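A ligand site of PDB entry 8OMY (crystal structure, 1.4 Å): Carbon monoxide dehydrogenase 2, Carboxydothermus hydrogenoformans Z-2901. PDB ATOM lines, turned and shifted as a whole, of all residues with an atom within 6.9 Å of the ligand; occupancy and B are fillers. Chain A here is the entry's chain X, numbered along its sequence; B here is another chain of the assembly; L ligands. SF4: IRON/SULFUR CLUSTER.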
ATOM      1  N   CYS A  47     -12.440   6.415 -13.832  1.00  0.00           N
ATOM      2  CA  CYS A  47     -13.209   5.784 -12.766  1.00  0.00           C
ATOM      3  C   CYS A  47     -12.297   4.817 -12.033  1.00  0.00           C
ATOM      4  O   CYS A  47     -11.455   4.158 -12.661  1.00  0.00           O
ATOM      5  CB  CYS A  47     -14.367   5.033 -13.365  1.00  0.00           C
ATOM      6  SG  CYS A  47     -15.350   4.181 -12.016  1.00  0.00           S
ATOM      7  N   CYS A  48     -12.415   4.827 -10.691  1.00  0.00           N
ATOM      8  CA  CYS A  48     -11.655   3.925  -9.857  1.00  0.00           C
ATOM      9  C   CYS A  48     -12.603   3.290  -8.865  1.00  0.00           C
ATOM     10  O   CYS A  48     -13.344   3.989  -8.158  1.00  0.00           O
ATOM     11  CB  CYS A  48     -10.513   4.687  -9.138  1.00  0.00           C
ATOM     12  SG  CYS A  48      -9.524   3.680  -8.098  1.00  0.00           S
ATOM     13  N   ARG A  49     -12.471   1.990  -8.685  1.00  0.00           N
ATOM     14  CA  ARG A  49     -13.158   1.192  -7.683  1.00  0.00           C
ATOM     15  C   ARG A  49     -12.158   0.377  -6.851  1.00  0.00           C
ATOM     16  O   ARG A  49     -12.456  -0.717  -6.388  1.00  0.00           O
ATOM     17  CB  ARG A  49     -14.226   0.289  -8.321  1.00  0.00           C
ATOM     18  CG  ARG A  49     -15.300   1.059  -8.993  1.00  0.00           C
ATOM     19  CD  ARG A  49     -16.176   0.165  -9.861  1.00  0.00           C
ATOM     20  NE  ARG A  49     -16.783  -0.849  -9.072  1.00  0.00           N
ATOM     21  CZ  ARG A  49     -17.212  -2.020  -9.491  1.00  0.00           C
ATOM     22  NH1 ARG A  49     -17.199  -2.360 -10.771  1.00  0.00           N
ATOM     23  NH2 ARG A  49     -17.733  -2.869  -8.599  1.00  0.00           N
ATOM     24  N   HIS A  50     -10.928   0.892  -6.707  1.00  0.00           N
ATOM     25  CA  HIS A  50      -9.874   0.135  -6.016  1.00  0.00           C
ATOM     26  C   HIS A  50     -10.003   0.143  -4.493  1.00  0.00           C
ATOM     27  O   HIS A  50      -9.254  -0.601  -3.846  1.00  0.00           O
ATOM     28  CB  HIS A  50      -8.484   0.527  -6.458  1.00  0.00           C
ATOM     29  CG  HIS A  50      -8.174   0.212  -7.884  1.00  0.00           C
ATOM     30  ND1 HIS A  50      -6.895   0.207  -8.386  1.00  0.00           N
ATOM     31  CD2 HIS A  50      -8.986  -0.101  -8.926  1.00  0.00           C
ATOM     32  CE1 HIS A  50      -6.940  -0.110  -9.678  1.00  0.00           C
ATOM     33  NE2 HIS A  50      -8.193  -0.303 -10.030  1.00  0.00           N
ATOM     34  N   CYS A  51     -10.983   0.829  -3.938  1.00  0.00           N
ATOM     35  CA  CYS A  51     -11.290   0.660  -2.517  1.00  0.00           C
ATOM     36  C   CYS A  51     -12.741   0.965  -2.247  1.00  0.00           C
ATOM     37  O   CYS A  51     -13.468   1.439  -3.118  1.00  0.00           O
ATOM     38  CB  CYS A  51     -10.356   1.454  -1.634  1.00  0.00           C
ATOM     39  SG  CYS A  51     -10.808   3.256  -1.441  1.00  0.00           S
ATOM     40  N   LEU A  52     -13.167   0.633  -1.024  1.00  0.00           N
ATOM     41  CA  LEU A  52     -14.561   0.772  -0.631  1.00  0.00           C
ATOM     42  C   LEU A  52     -14.974   2.200  -0.271  1.00  0.00           C
ATOM     43  O   LEU A  52     -16.136   2.440   0.095  1.00  0.00           O
ATOM     44  CB  LEU A  52     -14.882  -0.196   0.491  1.00  0.00           C
ATOM     45  CG  LEU A  52     -14.689  -1.665   0.166  1.00  0.00           C
ATOM     46  CD1 LEU A  52     -15.000  -2.500   1.420  1.00  0.00           C
ATOM     47  CD2 LEU A  52     -15.534  -2.090  -0.998  1.00  0.00           C
ATOM     48  N   GLN A  53     -14.088   3.158  -0.487  1.00  0.00           N
ATOM     49  CA  GLN A  53     -14.462   4.565  -0.477  1.00  0.00           C
ATOM     50  C   GLN A  53     -15.048   5.002  -1.794  1.00  0.00           C
ATOM     51  O   GLN A  53     -15.770   5.989  -1.850  1.00  0.00           O
ATOM     52  CB  GLN A  53     -13.324   5.518  -0.088  1.00  0.00           C
ATOM     53  CG  GLN A  53     -12.841   5.271   1.302  1.00  0.00           C
ATOM     54  CD  GLN A  53     -11.719   6.147   1.823  1.00  0.00           C
ATOM     55  OE1 GLN A  53     -11.687   6.481   2.989  1.00  0.00           O
ATOM     56  NE2 GLN A  53     -10.772   6.476   0.955  1.00  0.00           N
ATOM     57  N   GLY A  54     -14.773   4.244  -2.864  1.00  0.00           N
ATOM     58  CA  GLY A  54     -15.270   4.567  -4.192  1.00  0.00           C
ATOM     59  C   GLY A  54     -16.717   4.156  -4.347  1.00  0.00           C
ATOM     60  O   GLY A  54     -17.373   3.670  -3.397  1.00  0.00           O
ATOM     61  N   PRO A  55     -17.199   4.208  -5.536  1.00  0.00           N
ATOM     62  CA  PRO A  55     -16.472   4.545  -6.749  1.00  0.00           C
ATOM     63  C   PRO A  55     -16.121   6.010  -6.785  1.00  0.00           C
ATOM     64  O   PRO A  55     -16.853   6.894  -6.377  1.00  0.00           O
ATOM     65  CB  PRO A  55     -17.437   4.131  -7.881  1.00  0.00           C
ATOM     66  CG  PRO A  55     -18.653   3.834  -7.276  1.00  0.00           C
ATOM     67  CD  PRO A  55     -18.567   3.771  -5.793  1.00  0.00           C
ATOM     68  N   CYS A  56     -14.938   6.221  -7.335  1.00  0.00           N
ATOM     69  CA  CYS A  56     -14.477   7.575  -7.657  1.00  0.00           C
ATOM     70  C   CYS A  56     -14.481   7.803  -9.153  1.00  0.00           C
ATOM     71  O   CYS A  56     -14.136   6.902  -9.931  1.00  0.00           O
ATOM     72  CB  CYS A  56     -13.086   7.782  -7.126  1.00  0.00           C
ATOM     73  SG  CYS A  56     -13.038   7.865  -5.284  1.00  0.00           S
ATOM     74  N   ARG A  57     -14.897   8.958  -9.573  1.00  0.00           N
ATOM     75  CA  ARG A  57     -14.846   9.331 -10.969  1.00  0.00           C
ATOM     76  C   ARG A  57     -14.251  10.733 -11.010  1.00  0.00           C
ATOM     77  O   ARG A  57     -14.196  11.455  -9.993  1.00  0.00           O
ATOM     78  CB  ARG A  57     -16.202   9.266 -11.653  1.00  0.00           C
ATOM     79  CG  ARG A  57     -17.076  10.310 -11.108  1.00  0.00           C
ATOM     80  CD  ARG A  57     -18.579  10.042 -11.295  1.00  0.00           C
ATOM     81  NE  ARG A  57     -19.348  11.194 -10.801  1.00  0.00           N
ATOM     82  CZ  ARG A  57     -19.526  11.531  -9.523  1.00  0.00           C
ATOM     83  NH1 ARG A  57     -19.122  10.745  -8.502  1.00  0.00           N
ATOM     84  NH2 ARG A  57     -20.166  12.654  -9.252  1.00  0.00           N
ATOM     85  N   VAL A  67     -10.476  14.892  -8.614  1.00  0.00           N
ATOM     86  CA  VAL A  67      -9.456  14.039  -7.975  1.00  0.00           C
ATOM     87  C   VAL A  67     -10.192  12.966  -7.205  1.00  0.00           C
ATOM     88  O   VAL A  67     -11.295  13.189  -6.746  1.00  0.00           O
ATOM     89  CB  VAL A  67      -8.536  14.923  -7.097  1.00  0.00           C
ATOM     90  CG1 VAL A  67      -9.322  15.582  -6.020  1.00  0.00           C
ATOM     91  CG2 VAL A  67      -7.424  14.145  -6.582  1.00  0.00           C
ATOM     92  N   GLY A  68      -9.584  11.803  -7.098  1.00  0.00           N
ATOM     93  CA  GLY A  68     -10.168  10.739  -6.305  1.00  0.00           C
ATOM     94  C   GLY A  68     -10.161  11.074  -4.815  1.00  0.00           C
ATOM     95  O   GLY A  68      -9.434  11.965  -4.353  1.00  0.00           O
ATOM     96  N   ILE A  69     -10.949  10.321  -4.056  1.00  0.00           N
ATOM     97  CA  ILE A  69     -11.128  10.631  -2.628  1.00  0.00           C
ATOM     98  C   ILE A  69      -9.800  10.561  -1.871  1.00  0.00           C
ATOM     99  O   ILE A  69      -9.513  11.414  -1.017  1.00  0.00           O
ATOM    100  CB  ILE A  69     -12.223   9.748  -1.989  1.00  0.00           C
ATOM    101  CG1 ILE A  69     -13.586  10.176  -2.541  1.00  0.00           C
ATOM    102  CG2 ILE A  69     -12.178   9.767  -0.481  1.00  0.00           C
ATOM    103  CD1 ILE A  69     -14.723   9.221  -2.213  1.00  0.00           C
ATOM    104  N   CYS A  70      -8.929   9.591  -2.208  1.00  0.00           N
ATOM    105  CA  CYS A  70      -7.629   9.472  -1.529  1.00  0.00           C
ATOM    106  C   CYS A  70      -6.599  10.431  -2.047  1.00  0.00           C
ATOM    107  O   CYS A  70      -5.479  10.437  -1.534  1.00  0.00           O
ATOM    108  CB  CYS A  70      -7.122   8.073  -1.756  1.00  0.00           C
ATOM    109  SG  CYS A  70      -6.918   7.628  -3.495  1.00  0.00           S
ATOM    110  N   GLY A  71      -6.943  11.241  -3.058  1.00  0.00           N
ATOM    111  CA  GLY A  71      -5.988  12.112  -3.724  1.00  0.00           C
ATOM    112  C   GLY A  71      -5.489  11.591  -5.052  1.00  0.00           C
ATOM    113  O   GLY A  71      -4.625  12.235  -5.664  1.00  0.00           O
ATOM    114  N   ALA A  72      -5.937  10.424  -5.494  1.00  0.00           N
ATOM    115  CA  ALA A  72      -5.438   9.885  -6.768  1.00  0.00           C
ATOM    116  C   ALA A  72      -5.840  10.779  -7.927  1.00  0.00           C
ATOM    117  O   ALA A  72      -7.006  11.090  -8.097  1.00  0.00           O
ATOM    118  CB  ALA A  72      -5.985   8.497  -6.968  1.00  0.00           C
ATOM    119  N   THR A  73      -4.852  11.179  -8.687  1.00  0.00           N
ATOM    120  CA  THR A  73      -5.057  12.069  -9.829  1.00  0.00           C
ATOM    121  C   THR A  73      -5.615  11.290 -11.029  1.00  0.00           C
ATOM    122  O   THR A  73      -5.613  10.043 -11.043  1.00  0.00           O
ATOM    123  CB  THR A  73      -3.791  12.738 -10.246  1.00  0.00           C
ATOM    124  OG1 THR A  73      -2.913  11.700 -10.647  1.00  0.00           O
ATOM    125  CG2 THR A  73      -3.201  13.651  -9.154  1.00  0.00           C
ATOM    126  N   ILE A  77      -5.120   7.240 -11.692  1.00  0.00           N
ATOM    127  CA  ILE A  77      -6.277   6.376 -11.926  1.00  0.00           C
ATOM    128  C   ILE A  77      -6.206   5.726 -13.312  1.00  0.00           C
ATOM    129  O   ILE A  77      -6.335   4.493 -13.424  1.00  0.00           O
ATOM    130  CB  ILE A  77      -7.557   7.213 -11.762  1.00  0.00           C
ATOM    131  CG1 ILE A  77      -7.766   7.535 -10.271  1.00  0.00           C
ATOM    132  CG2 ILE A  77      -8.754   6.436 -12.283  1.00  0.00           C
ATOM    133  CD1 ILE A  77      -8.895   8.438  -9.960  1.00  0.00           C
ATOM    134  N   ARG A  80      -3.263   3.139 -13.331  1.00  0.00           N
ATOM    135  CA  ARG A  80      -3.564   1.939 -12.527  1.00  0.00           C
ATOM    136  C   ARG A  80      -4.548   1.023 -13.232  1.00  0.00           C
ATOM    137  O   ARG A  80      -4.355  -0.201 -13.220  1.00  0.00           O
ATOM    138  CB  ARG A  80      -4.119   2.315 -11.161  1.00  0.00           C
ATOM    139  CG  ARG A  80      -3.066   3.041 -10.298  1.00  0.00           C
ATOM    140  CD  ARG A  80      -3.455   3.180  -8.850  1.00  0.00           C
ATOM    141  NE  ARG A  80      -4.754   3.830  -8.682  1.00  0.00           N
ATOM    142  CZ  ARG A  80      -5.181   4.317  -7.526  1.00  0.00           C
ATOM    143  NH1 ARG A  80      -4.426   4.242  -6.444  1.00  0.00           N
ATOM    144  NH2 ARG A  80      -6.408   4.847  -7.432  1.00  0.00           N
ATOM    145  N   THR A 197      -0.978  -1.188  -7.740  1.00  0.00           N
ATOM    146  CA  THR A 197      -2.150  -0.482  -8.211  1.00  0.00           C
ATOM    147  C   THR A 197      -3.265  -0.439  -7.150  1.00  0.00           C
ATOM    148  O   THR A 197      -4.269   0.240  -7.367  1.00  0.00           O
ATOM    149  CB  THR A 197      -2.690  -1.082  -9.507  1.00  0.00           C
ATOM    150  OG1 THR A 197      -3.040  -2.444  -9.298  1.00  0.00           O
ATOM    151  CG2 THR A 197      -1.705  -0.889 -10.627  1.00  0.00           C
ATOM    152  N   SER A 198      -3.113  -1.135  -6.029  1.00  0.00           N
ATOM    153  CA  SER A 198      -4.088  -1.083  -4.953  1.00  0.00           C
ATOM    154  C   SER A 198      -3.965   0.265  -4.251  1.00  0.00           C
ATOM    155  O   SER A 198      -3.027   1.037  -4.470  1.00  0.00           O
ATOM    156  CB  SER A 198      -3.901  -2.301  -4.023  1.00  0.00           C
ATOM    157  OG  SER A 198      -2.770  -2.133  -3.191  1.00  0.00           O
ATOM    158  N   MET A 199      -4.997   0.594  -3.475  1.00  0.00           N
ATOM    159  CA  MET A 199      -5.093   1.900  -2.875  1.00  0.00           C
ATOM    160  C   MET A 199      -3.852   2.224  -2.031  1.00  0.00           C
ATOM    161  O   MET A 199      -3.319   1.405  -1.247  1.00  0.00           O
ATOM    162  CB  MET A 199      -6.212   1.973  -1.929  1.00  0.00           C
ATOM    163  CG  MET A 199      -6.662   3.326  -1.387  1.00  0.00           C
ATOM    164  SD  MET A 199      -5.717   3.494   0.225  1.00  0.00           S
ATOM    165  CE  MET A 199      -5.616   5.296   0.366  1.00  0.00           C
ATOM    166  N   GLY A 200      -3.372   3.453  -2.195  1.00  0.00           N
ATOM    167  CA  GLY A 200      -2.336   3.989  -1.342  1.00  0.00           C
ATOM    168  C   GLY A 200      -0.946   3.396  -1.579  1.00  0.00           C
ATOM    169  O   GLY A 200      -0.082   3.415  -0.689  1.00  0.00           O
ATOM    170  N   VAL B  28      -9.341  14.732   2.727  1.00  0.00           N
ATOM    171  CA  VAL B  28     -10.083  13.551   2.263  1.00  0.00           C
ATOM    172  C   VAL B  28     -11.599  13.748   2.381  1.00  0.00           C
ATOM    173  O   VAL B  28     -12.378  13.311   1.503  1.00  0.00           O
ATOM    174  CB  VAL B  28      -9.571  12.273   3.000  1.00  0.00           C
ATOM    175  CG1 VAL B  28      -9.870  12.326   4.489  1.00  0.00           C
ATOM    176  CG2 VAL B  28     -10.179  11.043   2.331  1.00  0.00           C
ATOM    177  N   MET B  35     -17.262  14.256  -4.415  1.00  0.00           N
ATOM    178  CA  MET B  35     -17.563  13.041  -5.192  1.00  0.00           C
ATOM    179  C   MET B  35     -19.037  12.677  -5.141  1.00  0.00           C
ATOM    180  O   MET B  35     -19.488  11.823  -5.932  1.00  0.00           O
ATOM    181  CB  MET B  35     -16.680  11.893  -4.709  1.00  0.00           C
ATOM    182  CG  MET B  35     -16.603  10.764  -5.630  1.00  0.00           C
ATOM    183  SD  MET B  35     -15.795  11.188  -7.193  1.00  0.00           S
ATOM    184  CE  MET B  35     -14.124  11.494  -6.673  1.00  0.00           C
ATOM    185  N   GLN B  38     -22.204   9.475  -5.420  1.00  0.00           N
ATOM    186  CA  GLN B  38     -21.356   8.482  -6.070  1.00  0.00           C
ATOM    187  C   GLN B  38     -22.181   7.561  -6.983  1.00  0.00           C
ATOM    188  O   GLN B  38     -23.387   7.370  -6.827  1.00  0.00           O
ATOM    189  CB  GLN B  38     -20.567   7.692  -5.029  1.00  0.00           C
ATOM    190  CG  GLN B  38     -19.545   8.497  -4.263  1.00  0.00           C
ATOM    191  CD  GLN B  38     -18.797   7.733  -3.235  1.00  0.00           C
ATOM    192  OE1 GLN B  38     -19.277   7.526  -2.126  1.00  0.00           O
ATOM    193  NE2 GLN B  38     -17.615   7.322  -3.579  1.00  0.00           N
ATOM    194  N   PRO B 336      -2.295   9.532  -1.557  1.00  0.00           N
ATOM    195  CA  PRO B 336      -1.286  10.273  -2.325  1.00  0.00           C
ATOM    196  C   PRO B 336      -1.425  11.785  -2.211  1.00  0.00           C
ATOM    197  O   PRO B 336      -0.500  12.540  -2.571  1.00  0.00           O
ATOM    198  CB  PRO B 336      -1.474   9.749  -3.749  1.00  0.00           C
ATOM    199  CG  PRO B 336      -2.877   9.235  -3.772  1.00  0.00           C
ATOM    200  CD  PRO B 336      -3.101   8.649  -2.391  1.00  0.00           C
ATOM    201  N   MET B 560     -12.054  -0.449   4.171  1.00  0.00           N
ATOM    202  CA  MET B 560     -11.724   0.367   3.009  1.00  0.00           C
ATOM    203  C   MET B 560     -10.944  -0.405   1.927  1.00  0.00           C
ATOM    204  O   MET B 560     -11.336  -0.489   0.768  1.00  0.00           O
ATOM    205  CB  MET B 560     -10.871   1.580   3.468  1.00  0.00           C
ATOM    206  CG  MET B 560     -10.645   2.470   2.339  1.00  0.00           C
ATOM    207  SD  MET B 560      -8.907   2.322   1.751  1.00  0.00           S
ATOM    208  CE  MET B 560      -7.960   2.767   3.100  1.00  0.00           C
HETATM  209 FE1  SF4 L   1     -11.280   6.392  -4.792  1.00  0.00          FE
HETATM  210 FE2  SF4 L   1     -10.354   4.325  -3.430  1.00  0.00          FE
HETATM  211 FE3  SF4 L   1      -9.800   4.628  -5.998  1.00  0.00          FE
HETATM  212 FE4  SF4 L   1      -8.684   6.299  -4.238  1.00  0.00          FE
HETATM  213  S1  SF4 L   1      -8.350   4.086  -4.452  1.00  0.00           S
HETATM  214  S2  SF4 L   1      -9.565   6.860  -6.157  1.00  0.00           S
HETATM  215  S3  SF4 L   1     -10.421   6.492  -2.798  1.00  0.00           S
HETATM  216  S4  SF4 L   1     -11.754   4.208  -5.109  1.00  0.00           S
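N of Gln 53 sits close to SG of Cys 51 (3.4 Å). The backbone carbonyl oxygen (O) of Cys 56 lies within hydrogen-bond range of the backbone NH (N) of Cys 48, 2.8 Å away. SG of Cys 48 lies close to NH2 of Arg 80. The backbone NH of His 50 sits close to the side-chain sulfur of Cys 48 (3.4 Å). N of Ile 69 sits close to SG of Cys 56. The backbone carbonyl oxygen (O) of Cys 56 sits close to the side-chain sulfur (SG) of Cys 47 (3.6 Å). The backbone carbonyl oxygen (O) of Gln 53 lies within hydrogen-bond range of the side-chain amide nitrogen (NE2) of Gln 38 of chain B (2.9 Å). ND1 of His 50 lies within hydrogen-bond range of O of Thr 197 (2.8 Å).
S4 of the ligand lies close to N of Cys 51 (3.7 Å). An iron atom (FE2) of the ligand is bound by the side-chain sulfur of Cys 51 (2.3 Å). An iron atom (FE3) of the ligand is bound by the side-chain sulfur (SG) of Cys 48 (2.3 Å). N of Cys 70 sits close to S3 of the ligand. FE4 of the ligand is bound by SG of Cys 70, at 2.3 Å. The side-chain sulfur (SG) of Cys 56 is bound to an iron atom (FE1) of the ligand. S1 of the ligand sits close to NH2 of Arg 80, at 3.6 Å. N of Gly 54 lies close to S4 of the ligand. The side-chain amide nitrogen (NE2) of Gln 53 lies close to a sulfur (S3) of the ligand (3.8 Å). S4 of the ligand lies close to N of His 50 (3.8 Å).
Merely in contact with the ligand: Met 199 (3.6 Å), Ile 69 (3.8 Å) and Gly 68 (3.9 Å). Hydrophobic or aromatic side chains that line the ligand: Ile 69 and Met 199. Within 4 Å of the ligand: Cys 48, His 50, Cys 51, Gln 53, Gly 54, Cys 56, Gly 68, Ile 69, Cys 70, Arg 80 and Met 199.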
